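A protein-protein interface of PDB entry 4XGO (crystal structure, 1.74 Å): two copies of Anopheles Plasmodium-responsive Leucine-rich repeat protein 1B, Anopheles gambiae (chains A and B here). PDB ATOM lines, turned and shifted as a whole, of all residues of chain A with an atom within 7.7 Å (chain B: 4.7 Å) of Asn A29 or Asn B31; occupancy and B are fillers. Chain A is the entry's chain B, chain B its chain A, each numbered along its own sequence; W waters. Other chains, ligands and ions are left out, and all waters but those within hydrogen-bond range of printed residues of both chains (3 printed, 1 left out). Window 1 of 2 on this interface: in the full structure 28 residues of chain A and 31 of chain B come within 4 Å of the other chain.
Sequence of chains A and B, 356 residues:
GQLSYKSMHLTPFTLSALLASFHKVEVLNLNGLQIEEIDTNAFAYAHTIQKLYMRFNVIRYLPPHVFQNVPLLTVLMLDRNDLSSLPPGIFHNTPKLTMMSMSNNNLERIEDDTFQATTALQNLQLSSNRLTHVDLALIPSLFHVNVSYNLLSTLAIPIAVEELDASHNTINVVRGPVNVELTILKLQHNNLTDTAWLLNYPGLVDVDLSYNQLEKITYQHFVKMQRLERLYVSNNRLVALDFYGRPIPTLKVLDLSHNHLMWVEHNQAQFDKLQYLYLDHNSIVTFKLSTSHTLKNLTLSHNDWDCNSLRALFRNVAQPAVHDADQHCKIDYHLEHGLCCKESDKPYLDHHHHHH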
ATOM      1  N   LEU A  18     -18.612 -12.334  24.336  1.00  0.00           N
ATOM      2  CA  LEU A  18     -18.940 -13.737  24.516  1.00  0.00           C
ATOM      3  C   LEU A  18     -17.802 -14.617  24.031  1.00  0.00           C
ATOM      4  O   LEU A  18     -17.376 -15.541  24.736  1.00  0.00           O
ATOM      5  CB  LEU A  18     -20.203 -14.101  23.752  1.00  0.00           C
ATOM      6  CG  LEU A  18     -21.532 -13.892  24.454  1.00  0.00           C
ATOM      7  CD1 LEU A  18     -22.651 -14.141  23.456  1.00  0.00           C
ATOM      8  CD2 LEU A  18     -21.652 -14.820  25.658  1.00  0.00           C
ATOM      9  N   SER A  21     -14.834 -14.779  26.362  1.00  0.00           N
ATOM     10  CA  SER A  21     -15.093 -15.627  27.519  1.00  0.00           C
ATOM     11  C   SER A  21     -15.058 -17.126  27.158  1.00  0.00           C
ATOM     12  O   SER A  21     -14.585 -17.945  27.947  1.00  0.00           O
ATOM     13  CB  SER A  21     -16.400 -15.221  28.189  1.00  0.00           C
ATOM     14  OG  SER A  21     -17.528 -15.605  27.423  1.00  0.00           O
ATOM     15  N   PHE A  22     -15.503 -17.470  25.953  1.00  0.00           N
ATOM     16  CA  PHE A  22     -15.382 -18.842  25.440  1.00  0.00           C
ATOM     17  C   PHE A  22     -13.919 -19.226  25.198  1.00  0.00           C
ATOM     18  O   PHE A  22     -13.463 -20.272  25.659  1.00  0.00           O
ATOM     19  CB  PHE A  22     -16.146 -19.024  24.126  1.00  0.00           C
ATOM     20  CG  PHE A  22     -17.639 -18.807  24.222  1.00  0.00           C
ATOM     21  CD1 PHE A  22     -18.315 -18.776  25.443  1.00  0.00           C
ATOM     22  CD2 PHE A  22     -18.375 -18.665  23.060  1.00  0.00           C
ATOM     23  CE1 PHE A  22     -19.696 -18.584  25.490  1.00  0.00           C
ATOM     24  CE2 PHE A  22     -19.751 -18.489  23.103  1.00  0.00           C
ATOM     25  CZ  PHE A  22     -20.410 -18.447  24.318  1.00  0.00           C
ATOM     26  N   GLU A  26     -13.635 -19.723  30.382  1.00  0.00           N
ATOM     27  CA  GLU A  26     -14.172 -19.188  31.629  1.00  0.00           C
ATOM     28  C   GLU A  26     -15.694 -19.326  31.639  1.00  0.00           C
ATOM     29  O   GLU A  26     -16.304 -19.465  32.682  1.00  0.00           O
ATOM     30  CB  GLU A  26     -13.789 -17.712  31.766  1.00  0.00           C
ATOM     31  CG  GLU A  26     -12.280 -17.522  31.799  1.00  0.00           C
ATOM     32  CD  GLU A  26     -11.840 -16.101  32.088  1.00  0.00           C
ATOM     33  OE1 GLU A  26     -12.702 -15.204  32.232  1.00  0.00           O
ATOM     34  OE2 GLU A  26     -10.609 -15.887  32.172  1.00  0.00           O
ATOM     35  N   VAL A  27     -16.282 -19.242  30.455  1.00  0.00           N
ATOM     36  CA  VAL A  27     -17.710 -19.434  30.270  1.00  0.00           C
ATOM     37  C   VAL A  27     -17.824 -20.577  29.278  1.00  0.00           C
ATOM     38  O   VAL A  27     -17.247 -20.528  28.188  1.00  0.00           O
ATOM     39  CB  VAL A  27     -18.397 -18.159  29.740  1.00  0.00           C
ATOM     40  CG1 VAL A  27     -19.880 -18.402  29.473  1.00  0.00           C
ATOM     41  CG2 VAL A  27     -18.219 -17.013  30.735  1.00  0.00           C
ATOM     42  N   LEU A  28     -18.541 -21.631  29.658  1.00  0.00           N
ATOM     43  CA  LEU A  28     -18.731 -22.766  28.772  1.00  0.00           C
ATOM     44  C   LEU A  28     -20.212 -22.918  28.465  1.00  0.00           C
ATOM     45  O   LEU A  28     -20.987 -23.253  29.352  1.00  0.00           O
ATOM     46  CB  LEU A  28     -18.216 -24.044  29.429  1.00  0.00           C
ATOM     47  CG  LEU A  28     -18.364 -25.331  28.630  1.00  0.00           C
ATOM     48  CD1 LEU A  28     -17.734 -25.203  27.247  1.00  0.00           C
ATOM     49  CD2 LEU A  28     -17.811 -26.525  29.400  1.00  0.00           C
ATOM     50  N   ASN A  29     -20.589 -22.662  27.213  1.00  0.00           N
ATOM     51  CA  ASN A  29     -21.979 -22.819  26.786  1.00  0.00           C
ATOM     52  C   ASN A  29     -22.222 -24.194  26.166  1.00  0.00           C
ATOM     53  O   ASN A  29     -21.810 -24.456  25.029  1.00  0.00           O
ATOM     54  CB  ASN A  29     -22.428 -21.696  25.820  1.00  0.00           C
ATOM     55  CG  ASN A  29     -23.917 -21.745  25.562  1.00  0.00           C
ATOM     56  OD1 ASN A  29     -24.651 -22.461  26.262  1.00  0.00           O
ATOM     57  ND2 ASN A  29     -24.378 -21.040  24.554  1.00  0.00           N
ATOM     58  N   LEU A  30     -22.878 -25.069  26.938  1.00  0.00           N
ATOM     59  CA  LEU A  30     -23.323 -26.382  26.475  1.00  0.00           C
ATOM     60  C   LEU A  30     -24.878 -26.430  26.417  1.00  0.00           C
ATOM     61  O   LEU A  30     -25.483 -27.508  26.419  1.00  0.00           O
ATOM     62  CB  LEU A  30     -22.801 -27.499  27.374  1.00  0.00           C
ATOM     63  CG  LEU A  30     -21.278 -27.587  27.556  1.00  0.00           C
ATOM     64  CD1 LEU A  30     -20.904 -28.618  28.602  1.00  0.00           C
ATOM     65  CD2 LEU A  30     -20.596 -27.933  26.247  1.00  0.00           C
ATOM     66  N   ASN A  31     -25.508 -25.259  26.350  1.00  0.00           N
ATOM     67  CA  ASN A  31     -26.964 -25.181  26.200  1.00  0.00           C
ATOM     68  C   ASN A  31     -27.432 -25.816  24.900  1.00  0.00           C
ATOM     69  O   ASN A  31     -26.794 -25.638  23.868  1.00  0.00           O
ATOM     70  CB  ASN A  31     -27.483 -23.745  26.152  1.00  0.00           C
ATOM     71  CG  ASN A  31     -27.335 -22.994  27.461  1.00  0.00           C
ATOM     72  OD1 ASN A  31     -27.078 -23.567  28.523  1.00  0.00           O
ATOM     73  ND2 ASN A  31     -27.505 -21.686  27.383  1.00  0.00           N
ATOM     74  N   GLY A  32     -28.547 -26.538  24.957  1.00  0.00           N
ATOM     75  CA  GLY A  32     -29.248 -26.940  23.745  1.00  0.00           C
ATOM     76  C   GLY A  32     -28.535 -27.937  22.855  1.00  0.00           C
ATOM     77  O   GLY A  32     -28.829 -27.989  21.660  1.00  0.00           O
ATOM     78  N   LEU A  33     -27.665 -28.776  23.439  1.00  0.00           N
ATOM     79  CA  LEU A  33     -26.901 -29.758  22.679  1.00  0.00           C
ATOM     80  C   LEU A  33     -27.443 -31.191  22.782  1.00  0.00           C
ATOM     81  O   LEU A  33     -26.750 -32.132  22.409  1.00  0.00           O
ATOM     82  CB  LEU A  33     -25.401 -29.702  23.080  1.00  0.00           C
ATOM     83  CG  LEU A  33     -24.679 -28.346  22.943  1.00  0.00           C
ATOM     84  CD1 LEU A  33     -23.258 -28.404  23.481  1.00  0.00           C
ATOM     85  CD2 LEU A  33     -24.679 -27.903  21.490  1.00  0.00           C
ATOM     86  N   GLN A  34     -28.681 -31.345  23.249  1.00  0.00           N
ATOM     87  CA  GLN A  34     -29.302 -32.650  23.444  1.00  0.00           C
ATOM     88  C   GLN A  34     -28.441 -33.612  24.268  1.00  0.00           C
ATOM     89  O   GLN A  34     -28.385 -34.817  23.989  1.00  0.00           O
ATOM     90  CB  GLN A  34     -29.692 -33.295  22.092  1.00  0.00           C
ATOM     91  CG  GLN A  34     -31.006 -32.818  21.482  1.00  0.00           C
ATOM     92  CD  GLN A  34     -32.204 -32.903  22.415  1.00  0.00           C
ATOM     93  OE1 GLN A  34     -32.464 -31.971  23.174  1.00  0.00           O
ATOM     94  NE2 GLN A  34     -32.978 -33.988  22.327  1.00  0.00           N
ATOM     95  N   ILE A  35     -27.818 -33.074  25.311  1.00  0.00           N
ATOM     96  CA  ILE A  35     -26.994 -33.870  26.202  1.00  0.00           C
ATOM     97  C   ILE A  35     -27.905 -34.687  27.091  1.00  0.00           C
ATOM     98  O   ILE A  35     -28.794 -34.147  27.745  1.00  0.00           O
ATOM     99  CB  ILE A  35     -26.058 -33.011  27.079  1.00  0.00           C
ATOM    100  CG1 ILE A  35     -25.051 -32.275  26.197  1.00  0.00           C
ATOM    101  CG2 ILE A  35     -25.334 -33.887  28.116  1.00  0.00           C
ATOM    102  CD1 ILE A  35     -24.321 -31.134  26.884  1.00  0.00           C
ATOM    103  N   LYS A  51     -18.471 -19.914  34.641  1.00  0.00           N
ATOM    104  CA  LYS A  51     -19.896 -19.992  34.309  1.00  0.00           C
ATOM    105  C   LYS A  51     -20.134 -21.194  33.431  1.00  0.00           C
ATOM    106  O   LYS A  51     -19.467 -21.361  32.414  1.00  0.00           O
ATOM    107  CB  LYS A  51     -20.374 -18.716  33.617  1.00  0.00           C
ATOM    108  CG  LYS A  51     -20.088 -17.470  34.432  1.00  0.00           C
ATOM    109  CD  LYS A  51     -20.803 -16.254  33.890  1.00  0.00           C
ATOM    110  CE  LYS A  51     -20.475 -15.014  34.696  1.00  0.00           C
ATOM    111  NZ  LYS A  51     -21.167 -13.829  34.109  1.00  0.00           N
ATOM    112  N   LEU A  52     -21.074 -22.045  33.840  1.00  0.00           N
ATOM    113  CA  LEU A  52     -21.345 -23.260  33.108  1.00  0.00           C
ATOM    114  C   LEU A  52     -22.823 -23.293  32.781  1.00  0.00           C
ATOM    115  O   LEU A  52     -23.654 -23.316  33.679  1.00  0.00           O
ATOM    116  CB  LEU A  52     -20.936 -24.483  33.937  1.00  0.00           C
ATOM    117  CG  LEU A  52     -21.218 -25.862  33.339  1.00  0.00           C
ATOM    118  CD1 LEU A  52     -20.569 -26.032  31.978  1.00  0.00           C
ATOM    119  CD2 LEU A  52     -20.718 -26.909  34.319  1.00  0.00           C
ATOM    120  N   TYR A  53     -23.114 -23.319  31.487  1.00  0.00           N
ATOM    121  CA  TYR A  53     -24.474 -23.311  30.984  1.00  0.00           C
ATOM    122  C   TYR A  53     -24.791 -24.662  30.341  1.00  0.00           C
ATOM    123  O   TYR A  53     -24.132 -25.073  29.383  1.00  0.00           O
ATOM    124  CB  TYR A  53     -24.638 -22.209  29.952  1.00  0.00           C
ATOM    125  CG  TYR A  53     -24.238 -20.819  30.375  1.00  0.00           C
ATOM    126  CD1 TYR A  53     -24.326 -20.396  31.699  1.00  0.00           C
ATOM    127  CD2 TYR A  53     -23.792 -19.903  29.426  1.00  0.00           C
ATOM    128  CE1 TYR A  53     -23.966 -19.115  32.067  1.00  0.00           C
ATOM    129  CE2 TYR A  53     -23.437 -18.619  29.787  1.00  0.00           C
ATOM    130  CZ  TYR A  53     -23.524 -18.225  31.106  1.00  0.00           C
ATOM    131  OH  TYR A  53     -23.162 -16.925  31.420  1.00  0.00           O
ATOM    132  N   MET A  54     -25.787 -25.350  30.900  1.00  0.00           N
ATOM    133  CA  MET A  54     -26.223 -26.651  30.396  1.00  0.00           C
ATOM    134  C   MET A  54     -27.760 -26.691  30.307  1.00  0.00           C
ATOM    135  O   MET A  54     -28.388 -27.716  30.550  1.00  0.00           O
ATOM    136  CB  MET A  54     -25.684 -27.783  31.289  1.00  0.00           C
ATOM    137  CG  MET A  54     -24.241 -28.165  31.002  1.00  0.00           C
ATOM    138  SD  MET A  54     -23.749 -29.668  31.865  1.00  0.00           S
ATOM    139  CE  MET A  54     -23.534 -28.973  33.506  1.00  0.00           C
ATOM    140  N   ARG A  55     -28.344 -25.561  29.933  1.00  0.00           N
ATOM    141  CA  ARG A  55     -29.789 -25.413  29.854  1.00  0.00           C
ATOM    142  C   ARG A  55     -30.334 -26.099  28.616  1.00  0.00           C
ATOM    143  O   ARG A  55     -29.638 -26.215  27.608  1.00  0.00           O
ATOM    144  CB  ARG A  55     -30.196 -23.924  29.766  1.00  0.00           C
ATOM    145  CG  ARG A  55     -29.501 -22.989  30.737  1.00  0.00           C
ATOM    146  CD  ARG A  55     -29.810 -21.545  30.408  1.00  0.00           C
ATOM    147  NE  ARG A  55     -31.192 -21.229  30.762  1.00  0.00           N
ATOM    148  CZ  ARG A  55     -31.925 -20.252  30.226  1.00  0.00           C
ATOM    149  NH1 ARG A  55     -31.450 -19.472  29.265  1.00  0.00           N
ATOM    150  NH2 ARG A  55     -33.168 -20.072  30.651  1.00  0.00           N
ATOM    151  N   PHE A  56     -31.598 -26.508  28.688  1.00  0.00           N
ATOM    152  CA  PHE A  56     -32.319 -27.004  27.517  1.00  0.00           C
ATOM    153  C   PHE A  56     -31.599 -28.216  26.936  1.00  0.00           C
ATOM    154  O   PHE A  56     -31.416 -28.322  25.723  1.00  0.00           O
ATOM    155  CB  PHE A  56     -32.457 -25.930  26.433  1.00  0.00           C
ATOM    156  CG  PHE A  56     -33.060 -24.651  26.919  1.00  0.00           C
ATOM    157  CD1 PHE A  56     -34.410 -24.575  27.194  1.00  0.00           C
ATOM    158  CD2 PHE A  56     -32.280 -23.527  27.068  1.00  0.00           C
ATOM    159  CE1 PHE A  56     -34.974 -23.373  27.617  1.00  0.00           C
ATOM    160  CE2 PHE A  56     -32.836 -22.329  27.505  1.00  0.00           C
ATOM    161  CZ  PHE A  56     -34.181 -22.280  27.798  1.00  0.00           C
ATOM    162  N   ASN A  57     -31.206 -29.130  27.808  1.00  0.00           N
ATOM    163  CA  ASN A  57     -30.737 -30.447  27.372  1.00  0.00           C
ATOM    164  C   ASN A  57     -31.758 -31.504  27.782  1.00  0.00           C
ATOM    165  O   ASN A  57     -32.948 -31.156  28.022  1.00  0.00           O
ATOM    166  CB  ASN A  57     -29.314 -30.686  27.893  1.00  0.00           C
ATOM    167  CG  ASN A  57     -28.288 -29.866  27.142  1.00  0.00           C
ATOM    168  OD1 ASN A  57     -27.995 -30.148  25.974  1.00  0.00           O
ATOM    169  ND2 ASN A  57     -27.701 -28.892  27.811  1.00  0.00           N
ATOM    170  N   PHE B  22     -15.065 -25.025  19.162  1.00  0.00           N
ATOM    171  CA  PHE B  22     -15.345 -23.704  19.695  1.00  0.00           C
ATOM    172  C   PHE B  22     -14.098 -22.830  19.577  1.00  0.00           C
ATOM    173  O   PHE B  22     -14.189 -21.665  19.202  1.00  0.00           O
ATOM    174  CB  PHE B  22     -15.718 -23.747  21.174  1.00  0.00           C
ATOM    175  CG  PHE B  22     -17.029 -24.430  21.481  1.00  0.00           C
ATOM    176  CD1 PHE B  22     -17.956 -24.739  20.482  1.00  0.00           C
ATOM    177  CD2 PHE B  22     -17.348 -24.730  22.801  1.00  0.00           C
ATOM    178  CE1 PHE B  22     -19.157 -25.338  20.804  1.00  0.00           C
ATOM    179  CE2 PHE B  22     -18.550 -25.330  23.120  1.00  0.00           C
ATOM    180  CZ  PHE B  22     -19.452 -25.632  22.122  1.00  0.00           C
ATOM    181  N   ASN B  29     -21.852 -21.767  19.582  1.00  0.00           N
ATOM    182  CA  ASN B  29     -23.045 -22.071  20.351  1.00  0.00           C
ATOM    183  C   ASN B  29     -23.593 -20.839  21.084  1.00  0.00           C
ATOM    184  O   ASN B  29     -23.067 -20.419  22.122  1.00  0.00           O
ATOM    185  CB  ASN B  29     -22.800 -23.223  21.320  1.00  0.00           C
ATOM    186  CG  ASN B  29     -24.082 -23.672  22.002  1.00  0.00           C
ATOM    187  OD1 ASN B  29     -25.171 -23.277  21.590  1.00  0.00           O
ATOM    188  ND2 ASN B  29     -23.966 -24.516  23.023  1.00  0.00           N
ATOM    189  N   LEU B  30     -24.657 -20.260  20.515  1.00  0.00           N
ATOM    190  CA  LEU B  30     -25.380 -19.172  21.124  1.00  0.00           C
ATOM    191  C   LEU B  30     -26.733 -19.650  21.613  1.00  0.00           C
ATOM    192  O   LEU B  30     -27.651 -18.850  21.840  1.00  0.00           O
ATOM    193  CB  LEU B  30     -25.561 -18.037  20.124  1.00  0.00           C
ATOM    194  CG  LEU B  30     -24.292 -17.447  19.533  1.00  0.00           C
ATOM    195  CD1 LEU B  30     -24.647 -16.343  18.528  1.00  0.00           C
ATOM    196  CD2 LEU B  30     -23.366 -16.938  20.623  1.00  0.00           C
ATOM    197  N   ASN B  31     -26.877 -20.957  21.806  1.00  0.00           N
ATOM    198  CA  ASN B  31     -28.154 -21.472  22.307  1.00  0.00           C
ATOM    199  C   ASN B  31     -28.430 -20.948  23.710  1.00  0.00           C
ATOM    200  O   ASN B  31     -27.514 -20.895  24.543  1.00  0.00           O
ATOM    201  CB  ASN B  31     -28.111 -22.988  22.429  1.00  0.00           C
ATOM    202  CG  ASN B  31     -28.050 -23.694  21.091  1.00  0.00           C
ATOM    203  OD1 ASN B  31     -28.282 -23.109  20.028  1.00  0.00           O
ATOM    204  ND2 ASN B  31     -27.715 -24.969  21.144  1.00  0.00           N
ATOM    205  N   GLY B  32     -29.685 -20.634  23.992  1.00  0.00           N
ATOM    206  CA  GLY B  32     -30.143 -20.419  25.358  1.00  0.00           C
ATOM    207  C   GLY B  32     -29.581 -19.169  26.027  1.00  0.00           C
ATOM    208  O   GLY B  32     -29.457 -19.135  27.251  1.00  0.00           O
ATOM    209  N   LEU B  33     -29.245 -18.147  25.228  1.00  0.00           N
ATOM    210  CA  LEU B  33     -28.640 -16.912  25.784  1.00  0.00           C
ATOM    211  C   LEU B  33     -29.612 -15.727  25.853  1.00  0.00           C
ATOM    212  O   LEU B  33     -29.177 -14.595  26.076  1.00  0.00           O
ATOM    213  CB  LEU B  33     -27.373 -16.537  25.023  1.00  0.00           C
ATOM    214  CG  LEU B  33     -26.254 -17.577  25.007  1.00  0.00           C
ATOM    215  CD1 LEU B  33     -25.062 -17.125  24.179  1.00  0.00           C
ATOM    216  CD2 LEU B  33     -25.808 -17.952  26.431  1.00  0.00           C
ATOM    217  N   TYR B  53     -25.429 -22.247  16.125  1.00  0.00           N
ATOM    218  CA  TYR B  53     -26.530 -22.703  16.964  1.00  0.00           C
ATOM    219  C   TYR B  53     -27.124 -21.528  17.718  1.00  0.00           C
ATOM    220  O   TYR B  53     -26.422 -20.885  18.512  1.00  0.00           O
ATOM    221  CB  TYR B  53     -26.059 -23.766  17.953  1.00  0.00           C
ATOM    222  CG  TYR B  53     -25.269 -24.921  17.394  1.00  0.00           C
ATOM    223  CD1 TYR B  53     -25.499 -25.408  16.120  1.00  0.00           C
ATOM    224  CD2 TYR B  53     -24.314 -25.572  18.190  1.00  0.00           C
ATOM    225  CE1 TYR B  53     -24.814 -26.497  15.629  1.00  0.00           C
ATOM    226  CE2 TYR B  53     -23.622 -26.678  17.718  1.00  0.00           C
ATOM    227  CZ  TYR B  53     -23.858 -27.131  16.445  1.00  0.00           C
ATOM    228  OH  TYR B  53     -23.180 -28.234  15.964  1.00  0.00           O
ATOM    229  N   MET B  54     -28.398 -21.214  17.438  1.00  0.00           N
ATOM    230  CA  MET B  54     -29.121 -20.134  18.136  1.00  0.00           C
ATOM    231  C   MET B  54     -30.497 -20.602  18.636  1.00  0.00           C
ATOM    232  O   MET B  54     -31.477 -19.839  18.686  1.00  0.00           O
ATOM    233  CB  MET B  54     -29.234 -18.886  17.232  1.00  0.00           C
ATOM    234  CG  MET B  54     -27.886 -18.345  16.824  1.00  0.00           C
ATOM    235  SD  MET B  54     -28.023 -16.803  15.878  1.00  0.00           S
ATOM    236  CE  MET B  54     -28.261 -17.442  14.251  1.00  0.00           C
ATOM    237  N   ARG B  55     -30.535 -21.858  19.063  1.00  0.00           N
ATOM    238  CA  ARG B  55     -31.755 -22.487  19.573  1.00  0.00           C
ATOM    239  C   ARG B  55     -32.094 -21.936  20.975  1.00  0.00           C
ATOM    240  O   ARG B  55     -31.209 -21.485  21.698  1.00  0.00           O
ATOM    241  CB  ARG B  55     -31.544 -24.004  19.736  1.00  0.00           C
ATOM    242  CG  ARG B  55     -30.973 -24.780  18.552  1.00  0.00           C
ATOM    243  CD  ARG B  55     -30.675 -26.234  18.967  1.00  0.00           C
ATOM    244  NE  ARG B  55     -31.911 -27.015  18.925  1.00  0.00           N
ATOM    245  CZ  ARG B  55     -32.231 -28.054  19.691  1.00  0.00           C
ATOM    246  NH1 ARG B  55     -31.435 -28.516  20.638  1.00  0.00           N
ATOM    247  NH2 ARG B  55     -33.407 -28.634  19.517  1.00  0.00           N
ATOM    248  N   ASN B  57     -33.755 -19.263  22.117  1.00  0.00           N
ATOM    249  CA  ASN B  57     -33.620 -17.848  22.404  1.00  0.00           C
ATOM    250  C   ASN B  57     -34.995 -17.208  22.268  1.00  0.00           C
ATOM    251  O   ASN B  57     -36.021 -17.896  22.339  1.00  0.00           O
ATOM    252  CB  ASN B  57     -32.567 -17.238  21.468  1.00  0.00           C
ATOM    253  CG  ASN B  57     -31.146 -17.570  21.890  1.00  0.00           C
ATOM    254  OD1 ASN B  57     -30.683 -17.154  22.968  1.00  0.00           O
ATOM    255  ND2 ASN B  57     -30.444 -18.304  21.052  1.00  0.00           N
HETATM  256  O   HOH W   1     -34.015 -30.676  21.318  1.00  0.00           O
HETATM  257  O   HOH W   2     -27.440 -27.172  18.944  1.00  0.00           O
HETATM  258  O   HOH W   3     -27.404 -19.369  29.472  1.00  0.00           O
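Printed residues of chain B that touch a printed residue of chain A: Phe B22, Asn B29, Asn B31, Gly B32, Leu B33 and Arg B55.
Hydrophobic or aromatic side chains of chain B that line the printed part of chain A: Phe B22 and Leu B33.
Among the printed residues, 15 pairs touch across the chains.
Among the printed residues, merely in contact across the chains: Leu A18 with Leu B33 (3.9 Å), Phe A22 with Asn B29 (3.96 Å), Asn A29 with Phe B22 (3.9 Å), Asn A29 with Leu B33 (3.9 Å), Leu A30 with Asn B29 (3.98 Å), Leu A33 with Asn B29 (3.8 Å) and Phe A56 with Gly B32 (3.9 Å).
The backbone carbonyl oxygen (O) of Gly A32 sits at hydrogen-bond distance from the side-chain amide nitrogen (ND2) of Asn B31, at 3.3 Å.
The side-chain amide nitrogen of Asn A29 sits at hydrogen-bond distance from the backbone carbonyl oxygen of Asn B31.
O of Gly A32 is in hydrogen-bond range of NH1 of Arg B55 (2.8 Å).
O of Asn B29 lies within hydrogen-bond range of ND2 of Asn A29 (2.8 Å).
The backbone carbonyl oxygen (O) of Asn B31 sits at hydrogen-bond distance from the side-chain amide nitrogen (ND2) of Asn A31 (2.9 Å).
The backbone carbonyl oxygen (O) of Asn A31 lies within hydrogen-bond range of the side-chain amide nitrogen (ND2) of Asn B29 (3.2 Å).
The side-chain amide nitrogen of Asn A31 sits at hydrogen-bond distance from the backbone carbonyl oxygen of Gly B32 (3.2 Å).
The backbone carbonyl oxygen of Gly B32 lies within hydrogen-bond range of the guanidinium group of Arg A55.
Water W1 bridges the side-chain amide oxygen (OE1) of Gln A34 (2.7 Å) and the guanidinium group (NH2) of Arg B55 (2.8 Å).
Water W3 bridges the backbone carbonyl oxygen (O) of Gly B32 (3.0 Å) and the side-chain amide nitrogen (ND2) of Asn A31 (3.1 Å).
Water W2 lies within hydrogen-bond range of ND2 of Asn B31 and O of Gly A32.
Phe A22 touches Asn B29, and with the chains exchanged Asn A29 touches Phe B22.
Leu A30 touches Asn B29, but with the chains exchanged Asn A29 does not touch Leu B30 (4.02 Å).
Asn A31 touches its own counterpart, Asn B31.
Asn A31 touches Gly B32, and with the chains exchanged Gly A32 touches Asn B31.
Positions printed for both chains: 22, 29, 30, 31, 32, 33, 53, 54, 55 and 57.
Of the 15 pairs that touch across the chains among the printed residues, 12 have their exchanged pair printed and touching as well.
N of Gly A32 is in hydrogen-bond range of O of Arg A55, 2.9 Å away.
The backbone NH (N) of Arg B55 lies within hydrogen-bond range of the side-chain amide oxygen (OD1) of Asn B31.
N of Asn B31 is in hydrogen-bond range of OD1 of Asn B29 (2.9 Å).
The side-chain amide oxygen of Asn B31 lies within hydrogen-bond range of the backbone NH of Met B54, at 3.2 Å.
The backbone NH of Asn A31 lies within hydrogen-bond range of the side-chain amide oxygen of Asn A29 (2.9 Å).
O of Tyr B53 lies close to OD1 of Asn B31 (3.3 Å).
Of the printed residues of chain B, Leu A18 touches Leu B33 (3.9 Å).
Glu A26 touches none of the printed residues of chain B.
Of the printed residues of chain B, Asn A29 touches Phe B22 (3.9 Å), Asn B29 (2.8 Å), Asn B31 (3.1 Å) and Leu B33 (3.9 Å).
Printed residues of chain B within 4 Å of Asn A31: Asn B29, Asn B31 and Gly B32.
Lys A51 touches none of the printed residues of chain B.
Of the printed residues of chain A, Phe B22 touches Asn A29.
Of the printed residues of chain A, Arg B55 touches Gly A32.
The nearest printed residue of chain B that does not touch Asn A29 is Leu B30 (4.02 Å).
The nearest residue of chain A that does not touch Asn B31 is Leu A33 (4.2 Å).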
